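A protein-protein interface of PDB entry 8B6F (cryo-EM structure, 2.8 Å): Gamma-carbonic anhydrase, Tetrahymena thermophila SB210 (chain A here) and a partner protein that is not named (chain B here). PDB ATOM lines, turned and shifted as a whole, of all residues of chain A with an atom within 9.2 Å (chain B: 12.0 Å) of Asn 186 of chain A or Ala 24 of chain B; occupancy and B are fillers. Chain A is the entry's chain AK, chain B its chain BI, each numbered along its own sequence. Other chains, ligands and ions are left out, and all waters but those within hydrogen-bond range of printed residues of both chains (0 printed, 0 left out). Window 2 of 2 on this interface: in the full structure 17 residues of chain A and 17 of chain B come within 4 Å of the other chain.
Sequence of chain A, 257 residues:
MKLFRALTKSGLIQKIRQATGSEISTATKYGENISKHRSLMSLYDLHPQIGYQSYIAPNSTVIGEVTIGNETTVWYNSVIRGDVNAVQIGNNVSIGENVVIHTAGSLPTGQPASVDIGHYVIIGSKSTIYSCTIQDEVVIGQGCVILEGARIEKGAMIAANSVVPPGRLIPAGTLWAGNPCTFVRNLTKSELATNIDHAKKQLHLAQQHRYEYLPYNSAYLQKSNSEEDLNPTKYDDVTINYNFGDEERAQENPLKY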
ATOM      1  N   GLU A 153      34.311 -21.398  -5.740  1.00  0.00           N
ATOM      2  CA  GLU A 153      34.696 -20.018  -5.973  1.00  0.00           C
ATOM      3  C   GLU A 153      34.600 -19.202  -4.684  1.00  0.00           C
ATOM      4  O   GLU A 153      34.192 -19.691  -3.630  1.00  0.00           O
ATOM      5  CB  GLU A 153      33.838 -19.412  -7.080  1.00  0.00           C
ATOM      6  CG  GLU A 153      34.080 -20.037  -8.442  1.00  0.00           C
ATOM      7  CD  GLU A 153      33.287 -19.360  -9.540  1.00  0.00           C
ATOM      8  OE1 GLU A 153      32.364 -18.584  -9.217  1.00  0.00           O
ATOM      9  OE2 GLU A 153      33.594 -19.595 -10.727  1.00  0.00           O
ATOM     10  N   LYS A 154      34.979 -17.929  -4.781  1.00  0.00           N
ATOM     11  CA  LYS A 154      35.114 -17.082  -3.604  1.00  0.00           C
ATOM     12  C   LYS A 154      33.790 -16.944  -2.859  1.00  0.00           C
ATOM     13  O   LYS A 154      32.753 -16.647  -3.458  1.00  0.00           O
ATOM     14  CB  LYS A 154      35.631 -15.707  -4.032  1.00  0.00           C
ATOM     15  CG  LYS A 154      35.778 -14.692  -2.911  1.00  0.00           C
ATOM     16  CD  LYS A 154      36.331 -13.380  -3.453  1.00  0.00           C
ATOM     17  CE  LYS A 154      36.468 -12.322  -2.368  1.00  0.00           C
ATOM     18  NZ  LYS A 154      35.165 -11.995  -1.726  1.00  0.00           N
ATOM     19  N   GLY A 155      33.833 -17.154  -1.545  1.00  0.00           N
ATOM     20  CA  GLY A 155      32.707 -16.876  -0.678  1.00  0.00           C
ATOM     21  C   GLY A 155      31.662 -17.965  -0.580  1.00  0.00           C
ATOM     22  O   GLY A 155      30.706 -17.807   0.188  1.00  0.00           O
ATOM     23  N   ALA A 156      31.804 -19.060  -1.318  1.00  0.00           N
ATOM     24  CA  ALA A 156      30.786 -20.097  -1.302  1.00  0.00           C
ATOM     25  C   ALA A 156      30.792 -20.847   0.028  1.00  0.00           C
ATOM     26  O   ALA A 156      31.788 -20.879   0.753  1.00  0.00           O
ATOM     27  CB  ALA A 156      31.004 -21.078  -2.452  1.00  0.00           C
ATOM     28  N   MET A 157      29.649 -21.455   0.342  1.00  0.00           N
ATOM     29  CA  MET A 157      29.478 -22.243   1.551  1.00  0.00           C
ATOM     30  C   MET A 157      28.947 -23.620   1.189  1.00  0.00           C
ATOM     31  O   MET A 157      28.250 -23.787   0.186  1.00  0.00           O
ATOM     32  CB  MET A 157      28.514 -21.571   2.534  1.00  0.00           C
ATOM     33  CG  MET A 157      29.082 -20.340   3.214  1.00  0.00           C
ATOM     34  SD  MET A 157      27.989 -19.670   4.479  1.00  0.00           S
ATOM     35  CE  MET A 157      27.988 -20.997   5.679  1.00  0.00           C
ATOM     36  N   PRO A 171      29.610 -21.804  -7.735  1.00  0.00           N
ATOM     37  CA  PRO A 171      29.801 -20.373  -7.985  1.00  0.00           C
ATOM     38  C   PRO A 171      30.095 -19.596  -6.712  1.00  0.00           C
ATOM     39  O   PRO A 171      29.807 -20.029  -5.595  1.00  0.00           O
ATOM     40  CB  PRO A 171      28.466 -19.932  -8.598  1.00  0.00           C
ATOM     41  CG  PRO A 171      27.840 -21.173  -9.098  1.00  0.00           C
ATOM     42  CD  PRO A 171      28.278 -22.256  -8.172  1.00  0.00           C
ATOM     43  N   ALA A 172      30.683 -18.419  -6.906  1.00  0.00           N
ATOM     44  CA  ALA A 172      31.059 -17.565  -5.789  1.00  0.00           C
ATOM     45  C   ALA A 172      29.828 -17.069  -5.041  1.00  0.00           C
ATOM     46  O   ALA A 172      28.805 -16.734  -5.642  1.00  0.00           O
ATOM     47  CB  ALA A 172      31.875 -16.376  -6.291  1.00  0.00           C
ATOM     48  N   GLY A 173      29.936 -17.020  -3.716  1.00  0.00           N
ATOM     49  CA  GLY A 173      28.875 -16.460  -2.892  1.00  0.00           C
ATOM     50  C   GLY A 173      27.561 -17.204  -2.981  1.00  0.00           C
ATOM     51  O   GLY A 173      26.498 -16.575  -3.031  1.00  0.00           O
ATOM     52  N   THR A 174      27.607 -18.532  -2.997  1.00  0.00           N
ATOM     53  CA  THR A 174      26.414 -19.358  -3.087  1.00  0.00           C
ATOM     54  C   THR A 174      26.454 -20.438  -2.017  1.00  0.00           C
ATOM     55  O   THR A 174      27.522 -20.831  -1.540  1.00  0.00           O
ATOM     56  CB  THR A 174      26.287 -19.990  -4.478  1.00  0.00           C
ATOM     57  OG1 THR A 174      27.451 -20.779  -4.754  1.00  0.00           O
ATOM     58  CG2 THR A 174      26.138 -18.925  -5.546  1.00  0.00           C
ATOM     59  N   LEU A 175      25.272 -20.915  -1.641  1.00  0.00           N
ATOM     60  CA  LEU A 175      25.115 -21.950  -0.629  1.00  0.00           C
ATOM     61  C   LEU A 175      24.681 -23.247  -1.294  1.00  0.00           C
ATOM     62  O   LEU A 175      23.753 -23.250  -2.109  1.00  0.00           O
ATOM     63  CB  LEU A 175      24.091 -21.526   0.426  1.00  0.00           C
ATOM     64  CG  LEU A 175      23.843 -22.498   1.581  1.00  0.00           C
ATOM     65  CD1 LEU A 175      25.112 -22.738   2.379  1.00  0.00           C
ATOM     66  CD2 LEU A 175      22.738 -21.977   2.477  1.00  0.00           C
ATOM     67  N   TRP A 176      25.351 -24.344  -0.947  1.00  0.00           N
ATOM     68  CA  TRP A 176      25.057 -25.661  -1.491  1.00  0.00           C
ATOM     69  C   TRP A 176      25.001 -26.674  -0.359  1.00  0.00           C
ATOM     70  O   TRP A 176      25.765 -26.582   0.605  1.00  0.00           O
ATOM     71  CB  TRP A 176      26.104 -26.080  -2.522  1.00  0.00           C
ATOM     72  CG  TRP A 176      26.130 -25.203  -3.729  1.00  0.00           C
ATOM     73  CD1 TRP A 176      26.591 -23.926  -3.799  1.00  0.00           C
ATOM     74  CD2 TRP A 176      25.688 -25.544  -5.050  1.00  0.00           C
ATOM     75  NE1 TRP A 176      26.460 -23.447  -5.077  1.00  0.00           N
ATOM     76  CE2 TRP A 176      25.908 -24.421  -5.865  1.00  0.00           C
ATOM     77  CE3 TRP A 176      25.124 -26.689  -5.619  1.00  0.00           C
ATOM     78  CZ2 TRP A 176      25.586 -24.404  -7.217  1.00  0.00           C
ATOM     79  CZ3 TRP A 176      24.803 -26.672  -6.964  1.00  0.00           C
ATOM     80  CH2 TRP A 176      25.035 -25.535  -7.748  1.00  0.00           C
ATOM     81  N   PHE A 183      22.005 -26.472  -5.101  1.00  0.00           N
ATOM     82  CA  PHE A 183      21.929 -25.053  -4.790  1.00  0.00           C
ATOM     83  C   PHE A 183      20.796 -24.775  -3.810  1.00  0.00           C
ATOM     84  O   PHE A 183      19.755 -25.437  -3.825  1.00  0.00           O
ATOM     85  CB  PHE A 183      21.724 -24.259  -6.080  1.00  0.00           C
ATOM     86  CG  PHE A 183      21.663 -22.775  -5.885  1.00  0.00           C
ATOM     87  CD1 PHE A 183      22.818 -22.046  -5.668  1.00  0.00           C
ATOM     88  CD2 PHE A 183      20.455 -22.104  -5.952  1.00  0.00           C
ATOM     89  CE1 PHE A 183      22.769 -20.679  -5.502  1.00  0.00           C
ATOM     90  CE2 PHE A 183      20.396 -20.737  -5.789  1.00  0.00           C
ATOM     91  CZ  PHE A 183      21.555 -20.023  -5.562  1.00  0.00           C
ATOM     92  N   VAL A 184      21.009 -23.779  -2.949  1.00  0.00           N
ATOM     93  CA  VAL A 184      20.012 -23.389  -1.958  1.00  0.00           C
ATOM     94  C   VAL A 184      19.623 -21.932  -2.170  1.00  0.00           C
ATOM     95  O   VAL A 184      18.450 -21.619  -2.401  1.00  0.00           O
ATOM     96  CB  VAL A 184      20.539 -23.613  -0.528  1.00  0.00           C
ATOM     97  CG1 VAL A 184      19.502 -23.194   0.504  1.00  0.00           C
ATOM     98  CG2 VAL A 184      20.932 -25.066  -0.324  1.00  0.00           C
ATOM     99  N   ARG A 185      20.598 -21.031  -2.089  1.00  0.00           N
ATOM    100  CA  ARG A 185      20.339 -19.607  -2.260  1.00  0.00           C
ATOM    101  C   ARG A 185      21.673 -18.881  -2.335  1.00  0.00           C
ATOM    102  O   ARG A 185      22.737 -19.472  -2.136  1.00  0.00           O
ATOM    103  CB  ARG A 185      19.487 -19.045  -1.118  1.00  0.00           C
ATOM    104  CG  ARG A 185      20.154 -19.126   0.250  1.00  0.00           C
ATOM    105  CD  ARG A 185      19.282 -18.501   1.325  1.00  0.00           C
ATOM    106  NE  ARG A 185      19.903 -18.572   2.643  1.00  0.00           N
ATOM    107  CZ  ARG A 185      20.766 -17.685   3.119  1.00  0.00           C
ATOM    108  NH1 ARG A 185      21.150 -16.640   2.404  1.00  0.00           N
ATOM    109  NH2 ARG A 185      21.255 -17.849   4.343  1.00  0.00           N
ATOM    110  N   ASN A 186      21.601 -17.587  -2.632  1.00  0.00           N
ATOM    111  CA  ASN A 186      22.779 -16.738  -2.614  1.00  0.00           C
ATOM    112  C   ASN A 186      23.091 -16.287  -1.189  1.00  0.00           C
ATOM    113  O   ASN A 186      22.225 -16.260  -0.312  1.00  0.00           O
ATOM    114  CB  ASN A 186      22.581 -15.516  -3.511  1.00  0.00           C
ATOM    115  CG  ASN A 186      22.415 -15.886  -4.965  1.00  0.00           C
ATOM    116  OD1 ASN A 186      22.949 -16.892  -5.426  1.00  0.00           O
ATOM    117  ND2 ASN A 186      21.671 -15.070  -5.700  1.00  0.00           N
ATOM    118  N   LEU A 187      24.350 -15.925  -0.971  1.00  0.00           N
ATOM    119  CA  LEU A 187      24.823 -15.456   0.322  1.00  0.00           C
ATOM    120  C   LEU A 187      24.995 -13.944   0.282  1.00  0.00           C
ATOM    121  O   LEU A 187      25.449 -13.387  -0.722  1.00  0.00           O
ATOM    122  CB  LEU A 187      26.143 -16.131   0.699  1.00  0.00           C
ATOM    123  CG  LEU A 187      26.069 -17.641   0.930  1.00  0.00           C
ATOM    124  CD1 LEU A 187      27.457 -18.216   1.098  1.00  0.00           C
ATOM    125  CD2 LEU A 187      25.212 -17.971   2.140  1.00  0.00           C
ATOM    126  N   THR A 188      24.633 -13.286   1.377  1.00  0.00           N
ATOM    127  CA  THR A 188      24.666 -11.834   1.457  1.00  0.00           C
ATOM    128  C   THR A 188      25.995 -11.352   2.030  1.00  0.00           C
ATOM    129  O   THR A 188      26.770 -12.114   2.608  1.00  0.00           O
ATOM    130  CB  THR A 188      23.509 -11.318   2.313  1.00  0.00           C
ATOM    131  OG1 THR A 188      23.588 -11.889   3.625  1.00  0.00           O
ATOM    132  CG2 THR A 188      22.177 -11.684   1.685  1.00  0.00           C
ATOM    133  N   LYS A 189      26.250 -10.052   1.863  1.00  0.00           N
ATOM    134  CA  LYS A 189      27.481  -9.467   2.384  1.00  0.00           C
ATOM    135  C   LYS A 189      27.611  -9.683   3.884  1.00  0.00           C
ATOM    136  O   LYS A 189      28.726  -9.839   4.394  1.00  0.00           O
ATOM    137  CB  LYS A 189      27.531  -7.976   2.057  1.00  0.00           C
ATOM    138  CG  LYS A 189      27.507  -7.673   0.570  1.00  0.00           C
ATOM    139  CD  LYS A 189      27.765  -6.198   0.309  1.00  0.00           C
ATOM    140  CE  LYS A 189      27.714  -5.877  -1.174  1.00  0.00           C
ATOM    141  NZ  LYS A 189      26.357  -6.101  -1.747  1.00  0.00           N
ATOM    142  N   SER A 190      26.491  -9.690   4.607  1.00  0.00           N
ATOM    143  CA  SER A 190      26.543  -9.961   6.038  1.00  0.00           C
ATOM    144  C   SER A 190      27.058 -11.370   6.310  1.00  0.00           C
ATOM    145  O   SER A 190      27.884 -11.573   7.207  1.00  0.00           O
ATOM    146  CB  SER A 190      25.163  -9.761   6.662  1.00  0.00           C
ATOM    147  OG  SER A 190      24.198 -10.583   6.034  1.00  0.00           O
ATOM    148  N   GLU A 191      26.578 -12.357   5.551  1.00  0.00           N
ATOM    149  CA  GLU A 191      27.064 -13.722   5.734  1.00  0.00           C
ATOM    150  C   GLU A 191      28.546 -13.824   5.403  1.00  0.00           C
ATOM    151  O   GLU A 191      29.306 -14.484   6.120  1.00  0.00           O
ATOM    152  CB  GLU A 191      26.258 -14.687   4.866  1.00  0.00           C
ATOM    153  CG  GLU A 191      24.762 -14.657   5.123  1.00  0.00           C
ATOM    154  CD  GLU A 191      24.397 -15.142   6.513  1.00  0.00           C
ATOM    155  OE1 GLU A 191      25.297 -15.621   7.236  1.00  0.00           O
ATOM    156  OE2 GLU A 191      23.208 -15.048   6.883  1.00  0.00           O
ATOM    157  N   LEU A 192      28.977 -13.182   4.316  1.00  0.00           N
ATOM    158  CA  LEU A 192      30.389 -13.211   3.952  1.00  0.00           C
ATOM    159  C   LEU A 192      31.243 -12.566   5.035  1.00  0.00           C
ATOM    160  O   LEU A 192      32.314 -13.078   5.383  1.00  0.00           O
ATOM    161  CB  LEU A 192      30.602 -12.515   2.609  1.00  0.00           C
ATOM    162  CG  LEU A 192      29.766 -13.047   1.443  1.00  0.00           C
ATOM    163  CD1 LEU A 192      30.041 -12.243   0.187  1.00  0.00           C
ATOM    164  CD2 LEU A 192      30.037 -14.522   1.200  1.00  0.00           C
ATOM    165  N   ALA B  24      27.902 -13.446  -5.211  1.00  0.00           N
ATOM    166  CA  ALA B  24      26.813 -14.173  -5.922  1.00  0.00           C
ATOM    167  C   ALA B  24      26.538 -13.527  -7.274  1.00  0.00           C
ATOM    168  O   ALA B  24      27.190 -12.556  -7.653  1.00  0.00           O
ATOM    169  CB  ALA B  24      25.550 -14.195  -5.079  1.00  0.00           C
ATOM    170  N   GLY B  25      25.563 -14.072  -7.996  1.00  0.00           N
ATOM    171  CA  GLY B  25      25.201 -13.549  -9.297  1.00  0.00           C
ATOM    172  C   GLY B  25      26.008 -14.167 -10.419  1.00  0.00           C
ATOM    173  O   GLY B  25      26.936 -14.958 -10.221  1.00  0.00           O
ATOM    174  N   ASN B  26      25.637 -13.783 -11.639  1.00  0.00           N
ATOM    175  CA  ASN B  26      26.282 -14.283 -12.849  1.00  0.00           C
ATOM    176  C   ASN B  26      26.133 -15.796 -12.976  1.00  0.00           C
ATOM    177  O   ASN B  26      26.983 -16.470 -13.561  1.00  0.00           O
ATOM    178  CB  ASN B  26      27.761 -13.885 -12.888  1.00  0.00           C
ATOM    179  CG  ASN B  26      28.378 -14.063 -14.263  1.00  0.00           C
ATOM    180  OD1 ASN B  26      27.674 -14.095 -15.271  1.00  0.00           O
ATOM    181  ND2 ASN B  26      29.699 -14.178 -14.307  1.00  0.00           N
ATOM    182  N   HIS B  27      25.053 -16.342 -12.422  1.00  0.00           N
ATOM    183  CA  HIS B  27      24.751 -17.761 -12.541  1.00  0.00           C
ATOM    184  C   HIS B  27      23.243 -17.924 -12.666  1.00  0.00           C
ATOM    185  O   HIS B  27      22.471 -17.036 -12.299  1.00  0.00           O
ATOM    186  CB  HIS B  27      25.309 -18.555 -11.347  1.00  0.00           C
ATOM    187  CG  HIS B  27      24.582 -18.315 -10.060  1.00  0.00           C
ATOM    188  ND1 HIS B  27      23.418 -18.971  -9.730  1.00  0.00           N
ATOM    189  CD2 HIS B  27      24.855 -17.493  -9.019  1.00  0.00           C
ATOM    190  CE1 HIS B  27      23.004 -18.566  -8.544  1.00  0.00           C
ATOM    191  NE2 HIS B  27      23.859 -17.669  -8.089  1.00  0.00           N
ATOM    192  N   HIS B  28      22.830 -19.077 -13.190  1.00  0.00           N
ATOM    193  CA  HIS B  28      21.421 -19.323 -13.477  1.00  0.00           C
ATOM    194  C   HIS B  28      20.936 -20.580 -12.771  1.00  0.00           C
ATOM    195  O   HIS B  28      20.269 -21.425 -13.377  1.00  0.00           O
ATOM    196  CB  HIS B  28      21.198 -19.449 -14.986  1.00  0.00           C
ATOM    197  CG  HIS B  28      21.694 -18.272 -15.765  1.00  0.00           C
ATOM    198  ND1 HIS B  28      21.051 -17.052 -15.762  1.00  0.00           N
ATOM    199  CD2 HIS B  28      22.769 -18.129 -16.576  1.00  0.00           C
ATOM    200  CE1 HIS B  28      21.710 -16.208 -16.534  1.00  0.00           C
ATOM    201  NE2 HIS B  28      22.756 -16.836 -17.040  1.00  0.00           N
ATOM    202  N   HIS B  29      21.269 -20.708 -11.495  1.00  0.00           N
ATOM    203  CA  HIS B  29      20.879 -21.851 -10.686  1.00  0.00           C
ATOM    204  C   HIS B  29      19.626 -21.531  -9.887  1.00  0.00           C
ATOM    205  O   HIS B  29      19.447 -20.406  -9.412  1.00  0.00           O
ATOM    206  CB  HIS B  29      22.009 -22.253  -9.735  1.00  0.00           C
ATOM    207  CG  HIS B  29      23.108 -23.019 -10.398  1.00  0.00           C
ATOM    208  ND1 HIS B  29      22.936 -24.300 -10.878  1.00  0.00           N
ATOM    209  CD2 HIS B  29      24.395 -22.692 -10.656  1.00  0.00           C
ATOM    210  CE1 HIS B  29      24.069 -24.726 -11.406  1.00  0.00           C
ATOM    211  NE2 HIS B  29      24.971 -23.769 -11.285  1.00  0.00           N
ATOM    212  N   HIS B  30      18.762 -22.529  -9.747  1.00  0.00           N
ATOM    213  CA  HIS B  30      17.576 -22.445  -8.914  1.00  0.00           C
ATOM    214  C   HIS B  30      17.689 -23.462  -7.788  1.00  0.00           C
ATOM    215  O   HIS B  30      18.477 -24.408  -7.857  1.00  0.00           O
ATOM    216  CB  HIS B  30      16.301 -22.695  -9.729  1.00  0.00           C
ATOM    217  CG  HIS B  30      16.090 -21.707 -10.832  1.00  0.00           C
ATOM    218  ND1 HIS B  30      15.675 -20.412 -10.601  1.00  0.00           N
ATOM    219  CD2 HIS B  30      16.234 -21.822 -12.173  1.00  0.00           C
ATOM    220  CE1 HIS B  30      15.574 -19.773 -11.753  1.00  0.00           C
ATOM    221  NE2 HIS B  30      15.908 -20.605 -12.722  1.00  0.00           N
ATOM    222  N   ALA B  31      16.898 -23.253  -6.742  1.00  0.00           N
ATOM    223  CA  ALA B  31      16.939 -24.130  -5.581  1.00  0.00           C
ATOM    224  C   ALA B  31      16.769 -25.581  -6.001  1.00  0.00           C
ATOM    225  O   ALA B  31      15.755 -25.951  -6.601  1.00  0.00           O
ATOM    226  CB  ALA B  31      15.846 -23.731  -4.588  1.00  0.00           C
ATOM    227  N   GLY B  32      17.767 -26.402  -5.688  1.00  0.00           N
ATOM    228  CA  GLY B  32      17.729 -27.813  -6.004  1.00  0.00           C
ATOM    229  C   GLY B  32      18.449 -28.226  -7.267  1.00  0.00           C
ATOM    230  O   GLY B  32      18.331 -29.389  -7.669  1.00  0.00           O
ATOM    231  N   ASP B  33      19.187 -27.324  -7.905  1.00  0.00           N
ATOM    232  CA  ASP B  33      19.900 -27.641  -9.132  1.00  0.00           C
ATOM    233  C   ASP B  33      21.292 -28.185  -8.827  1.00  0.00           C
ATOM    234  O   ASP B  33      21.877 -27.921  -7.775  1.00  0.00           O
ATOM    235  CB  ASP B  33      20.016 -26.405 -10.026  1.00  0.00           C
ATOM    236  CG  ASP B  33      18.689 -25.990 -10.622  1.00  0.00           C
ATOM    237  OD1 ASP B  33      17.831 -26.870 -10.837  1.00  0.00           O
ATOM    238  OD2 ASP B  33      18.504 -24.782 -10.876  1.00  0.00           O
ATOM    239  N   ASP B  36      27.361 -27.030 -12.274  1.00  0.00           N
ATOM    240  CA  ASP B  36      27.856 -27.217 -13.629  1.00  0.00           C
ATOM    241  C   ASP B  36      29.276 -27.768 -13.612  1.00  0.00           C
ATOM    242  O   ASP B  36      30.043 -27.550 -12.672  1.00  0.00           O
ATOM    243  CB  ASP B  36      27.827 -25.899 -14.402  1.00  0.00           C
ATOM    244  CG  ASP B  36      26.418 -25.401 -14.652  1.00  0.00           C
ATOM    245  OD1 ASP B  36      25.807 -24.849 -13.716  1.00  0.00           O
ATOM    246  OD2 ASP B  36      25.920 -25.564 -15.786  1.00  0.00           O
ATOM    247  N   GLU B  61      37.265 -17.251 -16.899  1.00  0.00           N
ATOM    248  CA  GLU B  61      36.896 -15.849 -17.010  1.00  0.00           C
ATOM    249  C   GLU B  61      37.024 -15.162 -15.656  1.00  0.00           C
ATOM    250  O   GLU B  61      36.664 -15.724 -14.619  1.00  0.00           O
ATOM    251  CB  GLU B  61      35.468 -15.710 -17.540  1.00  0.00           C
ATOM    252  CG  GLU B  61      34.409 -16.351 -16.662  1.00  0.00           C
ATOM    253  CD  GLU B  61      33.008 -16.118 -17.190  1.00  0.00           C
ATOM    254  OE1 GLU B  61      32.871 -15.431 -18.224  1.00  0.00           O
ATOM    255  OE2 GLU B  61      32.044 -16.619 -16.574  1.00  0.00           O
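Ala 24 of chain B touches Gly 173 of chain A. CG2 of Thr 174 of chain A touches NE2 of His 27 of chain B, 3.6 Å away. CH2 of Trp 176 of chain A touches CE1 of His 29 of chain B, at 3.9 Å. Trp 176 of chain A touches Asp 33 of chain B (CZ3 to O, 3.3 Å). CZ of Phe 183 of chain A touches CE1 of His 27 of chain B, at 3.6 Å. Phe 183 of chain A touches His 29 of chain B. O of His 30 of chain B touches CD2 of Phe 183 of chain A (3.6 Å). O of Phe 183 of chain A touches CA of Ala 31 of chain B (3.6 Å). CB of Ala 24 of chain B touches CG of Asn 186 of chain A, at 3.6 Å.
The backbone carbonyl oxygen of Lys 154 of chain A lies within hydrogen-bond range of the backbone NH of Gly 173 of chain A (2.9 Å). N of Met 157 of chain A sits at hydrogen-bond distance from O of Thr 174 of chain A, 2.9 Å away. N of Leu 187 of chain A sits at hydrogen-bond distance from O of Gly 173 of chain A, at 3.0 Å. NE1 of Trp 176 of chain A lies within hydrogen-bond range of OG1 of Thr 174 of chain A (2.9 Å). ND1 of His 27 of chain B sits at hydrogen-bond distance from N of His 29 of chain B (3.3 Å). OD2 of Asp 33 of chain B is in hydrogen-bond range of N of His 30 of chain B (2.5 Å).
O of Ala 172 of chain A sits close to N of Ala 24 of chain B (3.4 Å). The backbone NH (N) of Gly 32 of chain B sits at hydrogen-bond distance from the backbone carbonyl oxygen (O) of Phe 183 of chain A, at 2.9 Å. The backbone carbonyl oxygen (O) of Asp 33 of chain B lies within hydrogen-bond range of the backbone NH (N) of Phe 183 of chain A, at 3.0 Å. The side-chain amide oxygen (OD1) of Asn 186 of chain A is in hydrogen-bond range of a ring nitrogen (NE2) of His 27 of chain B, 2.9 Å away.
Pro 171 of chain A touches none of the printed residues of chain B. Of chain B, only Ala 24 comes within 4 Å of Ala 172 of chain A. Of chain B, only Ala 24 (3.3 Å) comes within 4 Å of Gly 173 of chain A. Of chain B, only His 27 comes within 4 Å of Thr 174 of chain A. Printed residues of chain B within 4 Å of Phe 183 of chain A: His 27 (3.6 Å), His 29 (3.8 Å), His 30 (3.6 Å), Ala 31 (3.6 Å), Gly 32 (2.9 Å) and Asp 33 (3.0 Å). No residue of chain B comes within 4 Å of Arg 185 of chain A. Asn 186 of chain A touches two residues of chain B. No residue of chain B comes within 4 Å of Leu 187 of chain A. No residue of chain B comes within 4 Å of Thr 188 of chain A. Ala 24 of chain B touches just these residues of chain A: Ala 172, Gly 173 and Asn 186. Of the printed residues of chain A, His 27 of chain B touches Thr 174 (3.6 Å), Phe 183 (3.6 Å) and Asn 186 (2.9 Å). The nearest printed residue of chain A that does not touch His 30 of chain B is Val 184 of chain A (5.6 Å).
Printed residues of chain B that touch a printed residue of chain A: Ala 24, His 27, His 29, His 30, Ala 31, Gly 32 and Asp 33. Hydrophobic or aromatic side chains of chain B that line the printed part of chain A: Ala 24, His 27 and His 29. Along chain B the printed residues that touch a printed residue of chain A span positions 24 to 33. Among the printed residues, no Asp or Glu carboxylate lies within 4 Å of a Lys or Arg side-chain nitrogen of the other chain.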
